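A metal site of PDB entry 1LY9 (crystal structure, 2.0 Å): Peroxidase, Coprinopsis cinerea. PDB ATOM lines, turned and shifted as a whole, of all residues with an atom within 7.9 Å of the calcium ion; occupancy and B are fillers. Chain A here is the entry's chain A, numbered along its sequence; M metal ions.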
ATOM      1  N   PRO A 129       4.578  14.860  31.317  1.00  0.00           N
ATOM      2  CA  PRO A 129       5.836  15.493  30.931  1.00  0.00           C
ATOM      3  C   PRO A 129       5.792  16.263  29.608  1.00  0.00           C
ATOM      4  O   PRO A 129       5.220  15.778  28.622  1.00  0.00           O
ATOM      5  CB  PRO A 129       6.809  14.323  30.875  1.00  0.00           C
ATOM      6  CG  PRO A 129       6.278  13.402  31.953  1.00  0.00           C
ATOM      7  CD  PRO A 129       4.787  13.454  31.727  1.00  0.00           C
ATOM      8  N   ALA A 181      -2.552  19.328  18.973  1.00  0.00           N
ATOM      9  CA  ALA A 181      -1.346  18.878  19.675  1.00  0.00           C
ATOM     10  C   ALA A 181      -1.770  17.966  20.822  1.00  0.00           C
ATOM     11  O   ALA A 181      -0.964  17.201  21.354  1.00  0.00           O
ATOM     12  CB  ALA A 181      -0.567  20.085  20.223  1.00  0.00           C
ATOM     13  N   ALA A 182      -3.035  18.049  21.213  1.00  0.00           N
ATOM     14  CA  ALA A 182      -3.558  17.211  22.284  1.00  0.00           C
ATOM     15  C   ALA A 182      -3.588  15.742  21.849  1.00  0.00           C
ATOM     16  O   ALA A 182      -3.730  14.842  22.693  1.00  0.00           O
ATOM     17  CB  ALA A 182      -4.954  17.668  22.685  1.00  0.00           C
ATOM     18  N   HIS A 183      -3.481  15.490  20.551  1.00  0.00           N
ATOM     19  CA  HIS A 183      -3.472  14.125  20.070  1.00  0.00           C
ATOM     20  C   HIS A 183      -2.096  13.507  20.332  1.00  0.00           C
ATOM     21  O   HIS A 183      -1.821  12.380  19.905  1.00  0.00           O
ATOM     22  CB  HIS A 183      -3.804  14.059  18.574  1.00  0.00           C
ATOM     23  CG  HIS A 183      -5.266  13.990  18.287  1.00  0.00           C
ATOM     24  ND1 HIS A 183      -5.798  13.576  17.089  1.00  0.00           N
ATOM     25  CD2 HIS A 183      -6.336  14.279  19.075  1.00  0.00           C
ATOM     26  CE1 HIS A 183      -7.138  13.624  17.175  1.00  0.00           C
ATOM     27  NE2 HIS A 183      -7.504  14.039  18.371  1.00  0.00           N
ATOM     28  N   SER A 184      -1.235  14.250  21.025  1.00  0.00           N
ATOM     29  CA  SER A 184       0.095  13.772  21.383  1.00  0.00           C
ATOM     30  C   SER A 184      -0.035  12.962  22.681  1.00  0.00           C
ATOM     31  O   SER A 184       0.914  12.319  23.114  1.00  0.00           O
ATOM     32  CB  SER A 184       1.052  14.951  21.622  1.00  0.00           C
ATOM     33  OG  SER A 184       2.382  14.511  21.824  1.00  0.00           O
ATOM     34  N   LEU A 185      -1.207  13.056  23.301  1.00  0.00           N
ATOM     35  CA  LEU A 185      -1.533  12.338  24.553  1.00  0.00           C
ATOM     36  C   LEU A 185      -2.857  11.656  24.249  1.00  0.00           C
ATOM     37  O   LEU A 185      -3.864  11.893  24.921  1.00  0.00           O
ATOM     38  CB  LEU A 185      -1.752  13.327  25.698  1.00  0.00           C
ATOM     39  CG  LEU A 185      -0.613  14.220  26.180  1.00  0.00           C
ATOM     40  CD1 LEU A 185      -1.127  15.157  27.270  1.00  0.00           C
ATOM     41  CD2 LEU A 185       0.523  13.374  26.708  1.00  0.00           C
ATOM     42  N   ALA A 186      -2.860  10.805  23.239  1.00  0.00           N
ATOM     43  CA  ALA A 186      -4.109  10.191  22.822  1.00  0.00           C
ATOM     44  C   ALA A 186      -4.083   8.740  22.360  1.00  0.00           C
ATOM     45  O   ALA A 186      -3.043   8.206  21.966  1.00  0.00           O
ATOM     46  CB  ALA A 186      -4.722  11.044  21.731  1.00  0.00           C
ATOM     47  N   LEU A 200      -2.032   7.300  19.442  1.00  0.00           N
ATOM     48  CA  LEU A 200      -2.001   8.089  18.219  1.00  0.00           C
ATOM     49  C   LEU A 200      -0.557   8.462  17.868  1.00  0.00           C
ATOM     50  O   LEU A 200      -0.258   8.807  16.718  1.00  0.00           O
ATOM     51  CB  LEU A 200      -2.880   9.335  18.361  1.00  0.00           C
ATOM     52  CG  LEU A 200      -4.295   9.216  17.763  1.00  0.00           C
ATOM     53  CD1 LEU A 200      -4.864   7.827  17.959  1.00  0.00           C
ATOM     54  CD2 LEU A 200      -5.200  10.261  18.384  1.00  0.00           C
ATOM     55  N   ASP A 201       0.312   8.414  18.866  1.00  0.00           N
ATOM     56  CA  ASP A 201       1.734   8.644  18.643  1.00  0.00           C
ATOM     57  C   ASP A 201       2.497   7.702  19.587  1.00  0.00           C
ATOM     58  O   ASP A 201       1.890   7.106  20.482  1.00  0.00           O
ATOM     59  CB  ASP A 201       2.129  10.140  18.786  1.00  0.00           C
ATOM     60  CG  ASP A 201       2.405  10.596  20.217  1.00  0.00           C
ATOM     61  OD1 ASP A 201       2.300   9.810  21.178  1.00  0.00           O
ATOM     62  OD2 ASP A 201       2.753  11.792  20.357  1.00  0.00           O
ATOM     63  N   SER A 202       3.795   7.543  19.362  1.00  0.00           N
ATOM     64  CA  SER A 202       4.598   6.621  20.163  1.00  0.00           C
ATOM     65  C   SER A 202       4.806   6.990  21.634  1.00  0.00           C
ATOM     66  O   SER A 202       5.395   6.205  22.381  1.00  0.00           O
ATOM     67  CB  SER A 202       5.961   6.398  19.493  1.00  0.00           C
ATOM     68  OG  SER A 202       6.715   7.602  19.487  1.00  0.00           O
ATOM     69  N   THR A 203       4.338   8.165  22.049  1.00  0.00           N
ATOM     70  CA  THR A 203       4.498   8.603  23.438  1.00  0.00           C
ATOM     71  C   THR A 203       3.171   9.161  23.971  1.00  0.00           C
ATOM     72  O   THR A 203       3.028  10.369  24.139  1.00  0.00           O
ATOM     73  CB  THR A 203       5.591   9.689  23.568  1.00  0.00           C
ATOM     74  OG1 THR A 203       5.297  10.776  22.667  1.00  0.00           O
ATOM     75  CG2 THR A 203       6.964   9.106  23.224  1.00  0.00           C
ATOM     76  N   PRO A 204       2.201   8.284  24.252  1.00  0.00           N
ATOM     77  CA  PRO A 204       0.897   8.720  24.748  1.00  0.00           C
ATOM     78  C   PRO A 204       0.920   9.358  26.125  1.00  0.00           C
ATOM     79  O   PRO A 204      -0.099   9.878  26.582  1.00  0.00           O
ATOM     80  CB  PRO A 204       0.057   7.440  24.697  1.00  0.00           C
ATOM     81  CG  PRO A 204       1.077   6.376  24.991  1.00  0.00           C
ATOM     82  CD  PRO A 204       2.246   6.810  24.133  1.00  0.00           C
ATOM     83  N   GLN A 205       2.081   9.339  26.789  1.00  0.00           N
ATOM     84  CA  GLN A 205       2.211   9.954  28.101  1.00  0.00           C
ATOM     85  C   GLN A 205       3.190  11.117  28.094  1.00  0.00           C
ATOM     86  O   GLN A 205       3.604  11.605  29.145  1.00  0.00           O
ATOM     87  CB  GLN A 205       2.653   8.931  29.150  1.00  0.00           C
ATOM     88  CG  GLN A 205       1.616   7.855  29.417  1.00  0.00           C
ATOM     89  CD  GLN A 205       2.034   6.932  30.532  1.00  0.00           C
ATOM     90  OE1 GLN A 205       2.959   6.137  30.380  1.00  0.00           O
ATOM     91  NE2 GLN A 205       1.351   7.034  31.671  1.00  0.00           N
ATOM     92  N   VAL A 206       3.568  11.555  26.898  1.00  0.00           N
ATOM     93  CA  VAL A 206       4.494  12.676  26.779  1.00  0.00           C
ATOM     94  C   VAL A 206       3.952  13.691  25.779  1.00  0.00           C
ATOM     95  O   VAL A 206       3.690  13.355  24.627  1.00  0.00           O
ATOM     96  CB  VAL A 206       5.908  12.229  26.303  1.00  0.00           C
ATOM     97  CG1 VAL A 206       6.852  13.420  26.288  1.00  0.00           C
ATOM     98  CG2 VAL A 206       6.443  11.143  27.205  1.00  0.00           C
ATOM     99  N   PHE A 207       3.776  14.916  26.241  1.00  0.00           N
ATOM    100  CA  PHE A 207       3.273  15.976  25.379  1.00  0.00           C
ATOM    101  C   PHE A 207       4.440  16.458  24.529  1.00  0.00           C
ATOM    102  O   PHE A 207       5.193  17.343  24.919  1.00  0.00           O
ATOM    103  CB  PHE A 207       2.722  17.122  26.219  1.00  0.00           C
ATOM    104  CG  PHE A 207       2.013  18.175  25.420  1.00  0.00           C
ATOM    105  CD1 PHE A 207       0.772  17.919  24.847  1.00  0.00           C
ATOM    106  CD2 PHE A 207       2.595  19.425  25.219  1.00  0.00           C
ATOM    107  CE1 PHE A 207       0.117  18.885  24.089  1.00  0.00           C
ATOM    108  CE2 PHE A 207       1.946  20.403  24.467  1.00  0.00           C
ATOM    109  CZ  PHE A 207       0.702  20.137  23.897  1.00  0.00           C
ATOM    110  N   ASP A 208       4.583  15.844  23.352  1.00  0.00           N
ATOM    111  CA  ASP A 208       5.683  16.179  22.450  1.00  0.00           C
ATOM    112  C   ASP A 208       5.224  16.275  20.993  1.00  0.00           C
ATOM    113  O   ASP A 208       4.030  16.197  20.702  1.00  0.00           O
ATOM    114  CB  ASP A 208       6.772  15.117  22.574  1.00  0.00           C
ATOM    115  CG  ASP A 208       6.231  13.704  22.425  1.00  0.00           C
ATOM    116  OD1 ASP A 208       5.102  13.562  21.909  1.00  0.00           O
ATOM    117  OD2 ASP A 208       6.933  12.746  22.821  1.00  0.00           O
ATOM    118  N   THR A 209       6.183  16.445  20.082  1.00  0.00           N
ATOM    119  CA  THR A 209       5.860  16.585  18.663  1.00  0.00           C
ATOM    120  C   THR A 209       5.775  15.273  17.890  1.00  0.00           C
ATOM    121  O   THR A 209       5.519  15.282  16.686  1.00  0.00           O
ATOM    122  CB  THR A 209       6.892  17.495  17.953  1.00  0.00           C
ATOM    123  OG1 THR A 209       8.180  16.866  17.962  1.00  0.00           O
ATOM    124  CG2 THR A 209       6.981  18.841  18.648  1.00  0.00           C
ATOM    125  N   GLN A 210       5.969  14.149  18.572  1.00  0.00           N
ATOM    126  CA  GLN A 210       5.917  12.858  17.903  1.00  0.00           C
ATOM    127  C   GLN A 210       4.648  12.681  17.093  1.00  0.00           C
ATOM    128  O   GLN A 210       4.683  12.131  16.001  1.00  0.00           O
ATOM    129  CB  GLN A 210       6.066  11.722  18.914  1.00  0.00           C
ATOM    130  CG  GLN A 210       7.426  11.725  19.600  1.00  0.00           C
ATOM    131  CD  GLN A 210       8.586  11.599  18.618  1.00  0.00           C
ATOM    132  OE1 GLN A 210       9.636  12.216  18.797  1.00  0.00           O
ATOM    133  NE2 GLN A 210       8.395  10.796  17.573  1.00  0.00           N
ATOM    134  N   PHE A 211       3.527  13.179  17.616  1.00  0.00           N
ATOM    135  CA  PHE A 211       2.251  13.058  16.914  1.00  0.00           C
ATOM    136  C   PHE A 211       2.329  13.675  15.517  1.00  0.00           C
ATOM    137  O   PHE A 211       1.861  13.086  14.537  1.00  0.00           O
ATOM    138  CB  PHE A 211       1.136  13.751  17.707  1.00  0.00           C
ATOM    139  CG  PHE A 211      -0.155  13.897  16.939  1.00  0.00           C
ATOM    140  CD1 PHE A 211      -0.925  12.777  16.616  1.00  0.00           C
ATOM    141  CD2 PHE A 211      -0.585  15.142  16.503  1.00  0.00           C
ATOM    142  CE1 PHE A 211      -2.090  12.897  15.867  1.00  0.00           C
ATOM    143  CE2 PHE A 211      -1.754  15.283  15.749  1.00  0.00           C
ATOM    144  CZ  PHE A 211      -2.504  14.149  15.434  1.00  0.00           C
ATOM    145  N   TYR A 212       2.920  14.860  15.409  1.00  0.00           N
ATOM    146  CA  TYR A 212       3.038  15.543  14.121  1.00  0.00           C
ATOM    147  C   TYR A 212       3.988  14.832  13.171  1.00  0.00           C
ATOM    148  O   TYR A 212       3.731  14.744  11.976  1.00  0.00           O
ATOM    149  CB  TYR A 212       3.501  16.995  14.341  1.00  0.00           C
ATOM    150  CG  TYR A 212       2.477  17.861  15.015  1.00  0.00           C
ATOM    151  CD1 TYR A 212       1.333  18.289  14.331  1.00  0.00           C
ATOM    152  CD2 TYR A 212       2.608  18.222  16.360  1.00  0.00           C
ATOM    153  CE1 TYR A 212       0.375  19.065  14.965  1.00  0.00           C
ATOM    154  CE2 TYR A 212       1.650  18.997  16.995  1.00  0.00           C
ATOM    155  CZ  TYR A 212       0.543  19.412  16.301  1.00  0.00           C
ATOM    156  OH  TYR A 212      -0.397  20.181  16.931  1.00  0.00           O
ATOM    157  N   GLU A 214       4.999  11.470  13.307  1.00  0.00           N
ATOM    158  CA  GLU A 214       4.508  10.142  12.960  1.00  0.00           C
ATOM    159  C   GLU A 214       3.295  10.102  12.033  1.00  0.00           C
ATOM    160  O   GLU A 214       3.159   9.164  11.242  1.00  0.00           O
ATOM    161  CB  GLU A 214       4.286   9.348  14.263  1.00  0.00           C
ATOM    162  CG  GLU A 214       5.600   9.249  15.052  1.00  0.00           C
ATOM    163  CD  GLU A 214       5.472   8.577  16.418  1.00  0.00           C
ATOM    164  OE1 GLU A 214       6.444   8.680  17.201  1.00  0.00           O
ATOM    165  OE2 GLU A 214       4.423   7.957  16.704  1.00  0.00           O
ATOM    166  N   ASN A 265       9.456  21.083  20.628  1.00  0.00           N
ATOM    167  CA  ASN A 265       8.453  20.856  21.673  1.00  0.00           C
ATOM    168  C   ASN A 265       8.074  22.212  22.266  1.00  0.00           C
ATOM    169  O   ASN A 265       6.924  22.457  22.611  1.00  0.00           O
ATOM    170  CB  ASN A 265       9.015  19.951  22.765  1.00  0.00           C
ATOM    171  CG  ASN A 265       9.135  18.505  22.324  1.00  0.00           C
ATOM    172  OD1 ASN A 265       8.204  17.938  21.746  1.00  0.00           O
ATOM    173  ND2 ASN A 265      10.267  17.888  22.618  1.00  0.00           N
ATOM    174  N   MET A 268       5.688  24.052  19.925  1.00  0.00           N
ATOM    175  CA  MET A 268       4.400  23.352  19.934  1.00  0.00           C
ATOM    176  C   MET A 268       3.627  23.750  21.192  1.00  0.00           C
ATOM    177  O   MET A 268       2.454  24.112  21.123  1.00  0.00           O
ATOM    178  CB  MET A 268       4.614  21.834  19.901  1.00  0.00           C
ATOM    179  CG  MET A 268       3.304  21.024  19.896  1.00  0.00           C
ATOM    180  SD  MET A 268       3.532  19.221  20.133  1.00  0.00           S
ATOM    181  CE  MET A 268       3.617  19.142  21.872  1.00  0.00           C
ATOM    182  N   ASN A 302      10.555  17.721  29.634  1.00  0.00           N
ATOM    183  CA  ASN A 302      10.787  16.654  28.662  1.00  0.00           C
ATOM    184  C   ASN A 302      12.062  17.072  27.949  1.00  0.00           C
ATOM    185  O   ASN A 302      12.044  18.012  27.149  1.00  0.00           O
ATOM    186  CB  ASN A 302       9.654  16.573  27.632  1.00  0.00           C
ATOM    187  CG  ASN A 302       9.956  15.583  26.513  1.00  0.00           C
ATOM    188  OD1 ASN A 302       9.410  15.681  25.418  1.00  0.00           O
ATOM    189  ND2 ASN A 302      10.826  14.616  26.807  1.00  0.00           N
HETATM  190 CA    CA M   1       3.257  12.137  22.635  1.00  0.00          CA
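The backbone NH (N) of Phe 211 lies close to the side-chain carboxylate (OD2) of Asp 201 (3.2 Å). N of Gln 210 lies close to OD1 of Asp 208, at 3.5 Å.
Of the 24 residues printed, 5 come within 4 Å of the calcium ion.
The calcium ion is bound by the backbone carbonyl oxygen of Thr 203 (2.3 Å), the side-chain carboxylate of Asp 201 (2.4 Å), the backbone carbonyl oxygen of Val 206 (2.4 Å), the backbone carbonyl oxygen of Ser 184 (2.4 Å), the side-chain carboxylate of Asp 208 (2.4 Å), the side-chain hydroxyl of Thr 203 (2.5 Å) and the side-chain hydroxyl of Ser 184 (2.7 Å). The calcium ion has seven donor atoms within binding distance. Slightly farther from the calcium ion lies the side-chain carboxylate (OD1) of Asp 201 (2.9 Å).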
